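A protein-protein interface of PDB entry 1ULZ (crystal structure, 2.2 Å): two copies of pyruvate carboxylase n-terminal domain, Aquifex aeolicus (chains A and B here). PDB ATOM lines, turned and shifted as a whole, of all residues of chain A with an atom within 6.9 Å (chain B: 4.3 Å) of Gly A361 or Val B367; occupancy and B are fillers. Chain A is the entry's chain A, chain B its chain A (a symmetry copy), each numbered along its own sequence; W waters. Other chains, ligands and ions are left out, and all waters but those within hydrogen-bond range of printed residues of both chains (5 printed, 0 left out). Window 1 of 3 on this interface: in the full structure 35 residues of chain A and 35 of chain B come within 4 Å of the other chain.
Of the printed residues of chain B, Pro A360 touches Arg B19 (3.5 Å).
Printed residues of chain B within 4 Å of Gly A361: Arg B19 and Val B367.
Printed residues of chain B within 4 Å of Gly A362: Arg B366 (3.4 Å), Val B367 (3.5 Å) and Glu B368 (3.1 Å).
Arg A366 touches none of the printed residues of chain B.
Of the printed residues of chain B, Thr A408 touches Arg B19 (2.9 Å).
Printed residues of chain A within 4 Å of Arg B366: Gly A362 and Phe A363.
Val B367 touches just these residues of chain A: Gly A361 (3.2 Å) and Gly A362 (3.5 Å).
Of the printed residues of chain A, His B369 touches Tyr A358 and Val A359.
The nearest printed residue of chain B that does not touch Gly A361 is Glu B368 (4.4 Å).
The nearest residue of chain A that does not touch Val B367 is Pro A360 (5.2 Å).
The nearest printed residue of chain B that does not touch Phe A363 is Glu B368 (4.02 Å).
5 positions are printed for both chains.
The side-chain hydroxyl of Tyr A358 sits at hydrogen-bond distance from the backbone carbonyl oxygen of His B369 (2.6 Å).
O of Val A359 is in hydrogen-bond range of NE2 of His B369, at 2.9 Å.
NE of Arg B19 sits at hydrogen-bond distance from O of Gly A361 (3.0 Å).
NH2 of Arg B19 lies within hydrogen-bond range of OG1 of Thr A408 (2.9 Å).
NE of Arg B366 lies close to N of Phe A363.
Among the printed residues, pairs that only touch across the chains: Gly A362 with Glu B368 (3.1 Å), Gly A361 with Val B367 (3.2 Å), Gly A362 with Arg B366 (3.4 Å), Pro A360 with Arg B19 (3.5 Å), Gly A362 with Val B367 (3.5 Å), Ala A405 with Arg B19 (3.6 Å) and Ile A365 with Arg B19 (3.6 Å).
Water W3 lies within hydrogen-bond range of NH1 of Arg B19 (2.9 Å) and N of Ala A405 (3.3 Å).
Water W1 lies within hydrogen-bond range of the guanidinium group (NH2) of Arg B19, the side-chain hydroxyl (OH) of Tyr A358 and the backbone NH (N) of Gly A361.
Water W2 lies within hydrogen-bond range of the backbone NH (N) of Gly A362 (2.9 Å), the backbone NH (N) of Val B367 (3.1 Å) and the backbone carbonyl oxygen (O) of Ile A365 (3.2 Å).
Water W5 lies within hydrogen-bond range of the backbone carbonyl oxygen (O) of Gly A361 (2.9 Å) and the side-chain carboxylate (OE1) of Glu B368 (3.0 Å).
Water W4 lies within hydrogen-bond range of N of His B369 and O of Gly A361.
Of the 12 printed residues of chain A, 9 touch a printed residue of chain B.
Printed residues of chain A that touch a printed residue of chain B: Tyr A358, Val A359, Pro A360, Gly A361, Gly A362, Phe A363, Ile A365, Ala A405 and Thr A408.
Printed residues of chain B that touch a printed residue of chain A: Arg B19, Arg B366, Val B367, Glu B368 and His B369.
Hydrophobic or aromatic side chains of chain B that line the printed part of chain A: His B369.
Along chain B the printed residues that touch a printed residue of chain A span positions 19 to 369.
The backbone carbonyl oxygen of Ala A405 is in hydrogen-bond range of the side-chain hydroxyl of Thr A408, 2.8 Å away.
OE2 of Glu B368 is in salt-bridge range of NE of Arg B366 (2.8 Å).
O of Glu B368 is in hydrogen-bond range of N of Lys B387, 2.9 Å away.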
ATOM      1  N   TYR A 358     -23.994  10.795  22.951  1.00  0.00           N
ATOM      2  CA  TYR A 358     -23.253   9.947  22.025  1.00  0.00           C
ATOM      3  C   TYR A 358     -24.162   9.558  20.867  1.00  0.00           C
ATOM      4  O   TYR A 358     -25.236   8.987  21.059  1.00  0.00           O
ATOM      5  CB  TYR A 358     -22.710   8.690  22.719  1.00  0.00           C
ATOM      6  CG  TYR A 358     -22.087   7.712  21.746  1.00  0.00           C
ATOM      7  CD1 TYR A 358     -22.806   6.616  21.275  1.00  0.00           C
ATOM      8  CD2 TYR A 358     -20.804   7.920  21.246  1.00  0.00           C
ATOM      9  CE1 TYR A 358     -22.269   5.755  20.335  1.00  0.00           C
ATOM     10  CE2 TYR A 358     -20.257   7.067  20.301  1.00  0.00           C
ATOM     11  CZ  TYR A 358     -20.997   5.985  19.846  1.00  0.00           C
ATOM     12  OH  TYR A 358     -20.478   5.155  18.881  1.00  0.00           O
ATOM     13  N   VAL A 359     -23.713   9.877  19.661  1.00  0.00           N
ATOM     14  CA  VAL A 359     -24.469   9.610  18.448  1.00  0.00           C
ATOM     15  C   VAL A 359     -24.067   8.286  17.814  1.00  0.00           C
ATOM     16  O   VAL A 359     -22.895   8.051  17.532  1.00  0.00           O
ATOM     17  CB  VAL A 359     -24.241  10.736  17.409  1.00  0.00           C
ATOM     18  CG1 VAL A 359     -25.118  10.510  16.190  1.00  0.00           C
ATOM     19  CG2 VAL A 359     -24.536  12.088  18.034  1.00  0.00           C
ATOM     20  N   PRO A 360     -25.043   7.393  17.595  1.00  0.00           N
ATOM     21  CA  PRO A 360     -24.752   6.094  16.983  1.00  0.00           C
ATOM     22  C   PRO A 360     -24.440   6.249  15.505  1.00  0.00           C
ATOM     23  O   PRO A 360     -24.919   7.185  14.855  1.00  0.00           O
ATOM     24  CB  PRO A 360     -26.032   5.299  17.226  1.00  0.00           C
ATOM     25  CG  PRO A 360     -27.095   6.358  17.215  1.00  0.00           C
ATOM     26  CD  PRO A 360     -26.449   7.475  18.025  1.00  0.00           C
ATOM     27  N   GLY A 361     -23.628   5.332  14.989  1.00  0.00           N
ATOM     28  CA  GLY A 361     -23.250   5.352  13.590  1.00  0.00           C
ATOM     29  C   GLY A 361     -22.924   3.955  13.087  1.00  0.00           C
ATOM     30  O   GLY A 361     -22.648   3.042  13.871  1.00  0.00           O
ATOM     31  N   GLY A 362     -22.960   3.784  11.771  1.00  0.00           N
ATOM     32  CA  GLY A 362     -22.667   2.492  11.188  1.00  0.00           C
ATOM     33  C   GLY A 362     -23.391   2.293   9.876  1.00  0.00           C
ATOM     34  O   GLY A 362     -24.029   3.213   9.357  1.00  0.00           O
ATOM     35  N   PHE A 363     -23.285   1.082   9.342  1.00  0.00           N
ATOM     36  CA  PHE A 363     -23.921   0.699   8.087  1.00  0.00           C
ATOM     37  C   PHE A 363     -25.446   0.882   8.185  1.00  0.00           C
ATOM     38  O   PHE A 363     -26.086   0.347   9.093  1.00  0.00           O
ATOM     39  CB  PHE A 363     -23.567  -0.766   7.794  1.00  0.00           C
ATOM     40  CG  PHE A 363     -24.123  -1.297   6.498  1.00  0.00           C
ATOM     41  CD1 PHE A 363     -25.490  -1.369   6.281  1.00  0.00           C
ATOM     42  CD2 PHE A 363     -23.269  -1.774   5.514  1.00  0.00           C
ATOM     43  CE1 PHE A 363     -25.996  -1.908   5.111  1.00  0.00           C
ATOM     44  CE2 PHE A 363     -23.768  -2.315   4.342  1.00  0.00           C
ATOM     45  CZ  PHE A 363     -25.130  -2.383   4.138  1.00  0.00           C
ATOM     46  N   ILE A 365     -27.105   3.597   8.910  1.00  0.00           N
ATOM     47  CA  ILE A 365     -27.526   4.550   9.926  1.00  0.00           C
ATOM     48  C   ILE A 365     -27.263   5.987   9.502  1.00  0.00           C
ATOM     49  O   ILE A 365     -26.163   6.322   9.061  1.00  0.00           O
ATOM     50  CB  ILE A 365     -26.794   4.299  11.266  1.00  0.00           C
ATOM     51  CG1 ILE A 365     -27.170   2.920  11.815  1.00  0.00           C
ATOM     52  CG2 ILE A 365     -27.133   5.406  12.270  1.00  0.00           C
ATOM     53  CD1 ILE A 365     -26.436   2.571  13.086  1.00  0.00           C
ATOM     54  N   ARG A 366     -28.281   6.830   9.644  1.00  0.00           N
ATOM     55  CA  ARG A 366     -28.182   8.241   9.297  1.00  0.00           C
ATOM     56  C   ARG A 366     -28.736   9.088  10.437  1.00  0.00           C
ATOM     57  O   ARG A 366     -29.778   8.766  11.017  1.00  0.00           O
ATOM     58  CB  ARG A 366     -28.962   8.527   8.011  1.00  0.00           C
ATOM     59  CG  ARG A 366     -29.041  10.006   7.637  1.00  0.00           C
ATOM     60  CD  ARG A 366     -29.770  10.197   6.315  1.00  0.00           C
ATOM     61  NE  ARG A 366     -30.050  11.605   6.045  1.00  0.00           N
ATOM     62  CZ  ARG A 366     -30.706  12.050   4.979  1.00  0.00           C
ATOM     63  NH1 ARG A 366     -31.160  11.197   4.068  1.00  0.00           N
ATOM     64  NH2 ARG A 366     -30.902  13.353   4.823  1.00  0.00           N
ATOM     65  N   VAL A 367     -28.039  10.168  10.761  1.00  0.00           N
ATOM     66  CA  VAL A 367     -28.483  11.044  11.832  1.00  0.00           C
ATOM     67  C   VAL A 367     -28.599  12.493  11.368  1.00  0.00           C
ATOM     68  O   VAL A 367     -27.668  13.038  10.776  1.00  0.00           O
ATOM     69  CB  VAL A 367     -27.515  10.995  13.046  1.00  0.00           C
ATOM     70  CG1 VAL A 367     -28.038  11.894  14.161  1.00  0.00           C
ATOM     71  CG2 VAL A 367     -27.359   9.556  13.543  1.00  0.00           C
ATOM     72  N   LEU A 388     -33.313  10.117  14.002  1.00  0.00           N
ATOM     73  CA  LEU A 388     -32.545   8.906  13.730  1.00  0.00           C
ATOM     74  C   LEU A 388     -33.235   8.095  12.638  1.00  0.00           C
ATOM     75  O   LEU A 388     -34.403   7.731  12.768  1.00  0.00           O
ATOM     76  CB  LEU A 388     -32.427   8.068  15.003  1.00  0.00           C
ATOM     77  CG  LEU A 388     -31.701   6.729  14.882  1.00  0.00           C
ATOM     78  CD1 LEU A 388     -30.246   6.948  14.454  1.00  0.00           C
ATOM     79  CD2 LEU A 388     -31.772   6.010  16.221  1.00  0.00           C
ATOM     80  N   ALA A 405     -29.623   0.871  17.173  1.00  0.00           N
ATOM     81  CA  ALA A 405     -29.117   2.239  17.139  1.00  0.00           C
ATOM     82  C   ALA A 405     -29.646   2.996  18.363  1.00  0.00           C
ATOM     83  O   ALA A 405     -28.891   3.675  19.057  1.00  0.00           O
ATOM     84  CB  ALA A 405     -29.560   2.929  15.851  1.00  0.00           C
ATOM     85  N   THR A 408     -28.033   2.314  21.654  1.00  0.00           N
ATOM     86  CA  THR A 408     -26.678   2.836  21.810  1.00  0.00           C
ATOM     87  C   THR A 408     -26.627   4.362  21.824  1.00  0.00           C
ATOM     88  O   THR A 408     -25.550   4.946  21.898  1.00  0.00           O
ATOM     89  CB  THR A 408     -25.751   2.351  20.678  1.00  0.00           C
ATOM     90  OG1 THR A 408     -26.210   2.876  19.424  1.00  0.00           O
ATOM     91  CG2 THR A 408     -25.734   0.835  20.612  1.00  0.00           C
ATOM     92  N   ARG B  19     -22.288  -3.637  17.285  1.00  0.00           N
ATOM     93  CA  ARG B  19     -23.511  -3.260  16.582  1.00  0.00           C
ATOM     94  C   ARG B  19     -23.993  -4.392  15.674  1.00  0.00           C
ATOM     95  O   ARG B  19     -25.187  -4.688  15.618  1.00  0.00           O
ATOM     96  CB  ARG B  19     -23.305  -1.987  15.748  1.00  0.00           C
ATOM     97  CG  ARG B  19     -24.566  -1.571  14.998  1.00  0.00           C
ATOM     98  CD  ARG B  19     -24.448  -0.205  14.355  1.00  0.00           C
ATOM     99  NE  ARG B  19     -24.147   0.842  15.323  1.00  0.00           N
ATOM    100  CZ  ARG B  19     -24.903   1.137  16.376  1.00  0.00           C
ATOM    101  NH1 ARG B  19     -26.018   0.461  16.613  1.00  0.00           N
ATOM    102  NH2 ARG B  19     -24.545   2.115  17.192  1.00  0.00           N
ATOM    103  N   VAL B 359     -20.745  15.672  15.740  1.00  0.00           N
ATOM    104  CA  VAL B 359     -20.653  14.719  14.646  1.00  0.00           C
ATOM    105  C   VAL B 359     -21.570  15.096  13.491  1.00  0.00           C
ATOM    106  O   VAL B 359     -22.771  15.278  13.672  1.00  0.00           O
ATOM    107  CB  VAL B 359     -21.040  13.299  15.132  1.00  0.00           C
ATOM    108  CG1 VAL B 359     -20.836  12.290  14.016  1.00  0.00           C
ATOM    109  CG2 VAL B 359     -20.215  12.923  16.350  1.00  0.00           C
ATOM    110  N   PRO B 360     -21.004  15.234  12.284  1.00  0.00           N
ATOM    111  CA  PRO B 360     -21.808  15.589  11.112  1.00  0.00           C
ATOM    112  C   PRO B 360     -22.672  14.419  10.673  1.00  0.00           C
ATOM    113  O   PRO B 360     -22.317  13.256  10.894  1.00  0.00           O
ATOM    114  CB  PRO B 360     -20.759  15.959  10.067  1.00  0.00           C
ATOM    115  CG  PRO B 360     -19.593  15.090  10.436  1.00  0.00           C
ATOM    116  CD  PRO B 360     -19.569  15.205  11.955  1.00  0.00           C
ATOM    117  N   ARG B 366     -21.643   8.667   6.762  1.00  0.00           N
ATOM    118  CA  ARG B 366     -21.561   7.588   7.737  1.00  0.00           C
ATOM    119  C   ARG B 366     -20.404   7.852   8.694  1.00  0.00           C
ATOM    120  O   ARG B 366     -19.315   8.259   8.275  1.00  0.00           O
ATOM    121  CB  ARG B 366     -21.354   6.247   7.029  1.00  0.00           C
ATOM    122  CG  ARG B 366     -21.113   5.068   7.970  1.00  0.00           C
ATOM    123  CD  ARG B 366     -20.987   3.765   7.192  1.00  0.00           C
ATOM    124  NE  ARG B 366     -20.542   2.665   8.041  1.00  0.00           N
ATOM    125  CZ  ARG B 366     -20.316   1.428   7.611  1.00  0.00           C
ATOM    126  NH1 ARG B 366     -20.492   1.121   6.331  1.00  0.00           N
ATOM    127  NH2 ARG B 366     -19.918   0.495   8.467  1.00  0.00           N
ATOM    128  N   VAL B 367     -20.638   7.622   9.979  1.00  0.00           N
ATOM    129  CA  VAL B 367     -19.599   7.839  10.972  1.00  0.00           C
ATOM    130  C   VAL B 367     -19.370   6.600  11.832  1.00  0.00           C
ATOM    131  O   VAL B 367     -20.317   6.026  12.371  1.00  0.00           O
ATOM    132  CB  VAL B 367     -19.949   9.027  11.910  1.00  0.00           C
ATOM    133  CG1 VAL B 367     -18.817   9.247  12.909  1.00  0.00           C
ATOM    134  CG2 VAL B 367     -20.197  10.296  11.091  1.00  0.00           C
ATOM    135  N   GLU B 368     -18.109   6.185  11.929  1.00  0.00           N
ATOM    136  CA  GLU B 368     -17.706   5.038  12.744  1.00  0.00           C
ATOM    137  C   GLU B 368     -16.867   5.584  13.902  1.00  0.00           C
ATOM    138  O   GLU B 368     -15.730   6.000  13.700  1.00  0.00           O
ATOM    139  CB  GLU B 368     -16.847   4.066  11.926  1.00  0.00           C
ATOM    140  CG  GLU B 368     -17.551   3.332  10.795  1.00  0.00           C
ATOM    141  CD  GLU B 368     -18.583   2.322  11.275  1.00  0.00           C
ATOM    142  OE1 GLU B 368     -18.315   1.610  12.271  1.00  0.00           O
ATOM    143  OE2 GLU B 368     -19.658   2.232  10.644  1.00  0.00           O
ATOM    144  N   HIS B 369     -17.412   5.598  15.113  1.00  0.00           N
ATOM    145  CA  HIS B 369     -16.646   6.126  16.239  1.00  0.00           C
ATOM    146  C   HIS B 369     -17.109   5.652  17.613  1.00  0.00           C
ATOM    147  O   HIS B 369     -18.173   5.048  17.766  1.00  0.00           O
ATOM    148  CB  HIS B 369     -16.679   7.660  16.226  1.00  0.00           C
ATOM    149  CG  HIS B 369     -18.000   8.237  16.636  1.00  0.00           C
ATOM    150  ND1 HIS B 369     -18.142   9.536  17.070  1.00  0.00           N
ATOM    151  CD2 HIS B 369     -19.232   7.680  16.710  1.00  0.00           C
ATOM    152  CE1 HIS B 369     -19.404   9.754  17.400  1.00  0.00           C
ATOM    153  NE2 HIS B 369     -20.085   8.642  17.192  1.00  0.00           N
ATOM    154  N   LYS B 387     -13.872   7.612  12.125  1.00  0.00           N
ATOM    155  CA  LYS B 387     -13.682   7.342  10.709  1.00  0.00           C
ATOM    156  C   LYS B 387     -14.888   7.940  10.003  1.00  0.00           C
ATOM    157  O   LYS B 387     -16.012   7.469  10.177  1.00  0.00           O
ATOM    158  CB  LYS B 387     -13.611   5.841  10.425  1.00  0.00           C
ATOM    159  CG  LYS B 387     -12.378   5.162  10.985  1.00  0.00           C
ATOM    160  CD  LYS B 387     -12.254   3.728  10.496  1.00  0.00           C
ATOM    161  CE  LYS B 387     -13.455   2.888  10.887  1.00  0.00           C
ATOM    162  NZ  LYS B 387     -13.194   1.436  10.684  1.00  0.00           N
ATOM    163  N   LEU B 388     -14.647   8.991   9.227  1.00  0.00           N
ATOM    164  CA  LEU B 388     -15.707   9.665   8.485  1.00  0.00           C
ATOM    165  C   LEU B 388     -15.743   9.140   7.052  1.00  0.00           C
ATOM    166  O   LEU B 388     -14.743   9.195   6.337  1.00  0.00           O
ATOM    167  CB  LEU B 388     -15.462  11.173   8.478  1.00  0.00           C
ATOM    168  CG  LEU B 388     -16.449  12.031   7.689  1.00  0.00           C
ATOM    169  CD1 LEU B 388     -17.859  11.894   8.273  1.00  0.00           C
ATOM    170  CD2 LEU B 388     -15.982  13.478   7.726  1.00  0.00           C
ATOM    171  N   TYR B 409     -17.367  19.260  11.210  1.00  0.00           N
ATOM    172  CA  TYR B 409     -16.979  18.364  12.301  1.00  0.00           C
ATOM    173  C   TYR B 409     -16.221  19.128  13.380  1.00  0.00           C
ATOM    174  O   TYR B 409     -15.028  19.394  13.231  1.00  0.00           O
ATOM    175  CB  TYR B 409     -16.100  17.241  11.745  1.00  0.00           C
ATOM    176  CG  TYR B 409     -16.182  15.907  12.467  1.00  0.00           C
ATOM    177  CD1 TYR B 409     -16.014  14.716  11.766  1.00  0.00           C
ATOM    178  CD2 TYR B 409     -16.417  15.831  13.832  1.00  0.00           C
ATOM    179  CE1 TYR B 409     -16.081  13.490  12.397  1.00  0.00           C
ATOM    180  CE2 TYR B 409     -16.482  14.597  14.481  1.00  0.00           C
ATOM    181  CZ  TYR B 409     -16.315  13.432  13.750  1.00  0.00           C
ATOM    182  OH  TYR B 409     -16.390  12.203  14.362  1.00  0.00           O
HETATM  183  O   HOH W   1     -22.092   3.642  16.898  1.00  0.00           O
HETATM  184  O   HOH W   2     -23.415   6.438  10.624  1.00  0.00           O
HETATM  185  O   HOH W   3     -27.878  -0.462  14.649  1.00  0.00           O
HETATM  186  O   HOH W   4     -19.831   3.668  15.373  1.00  0.00           O
HETATM  187  O   HOH W   5     -20.984   0.700  13.276  1.00  0.00           O
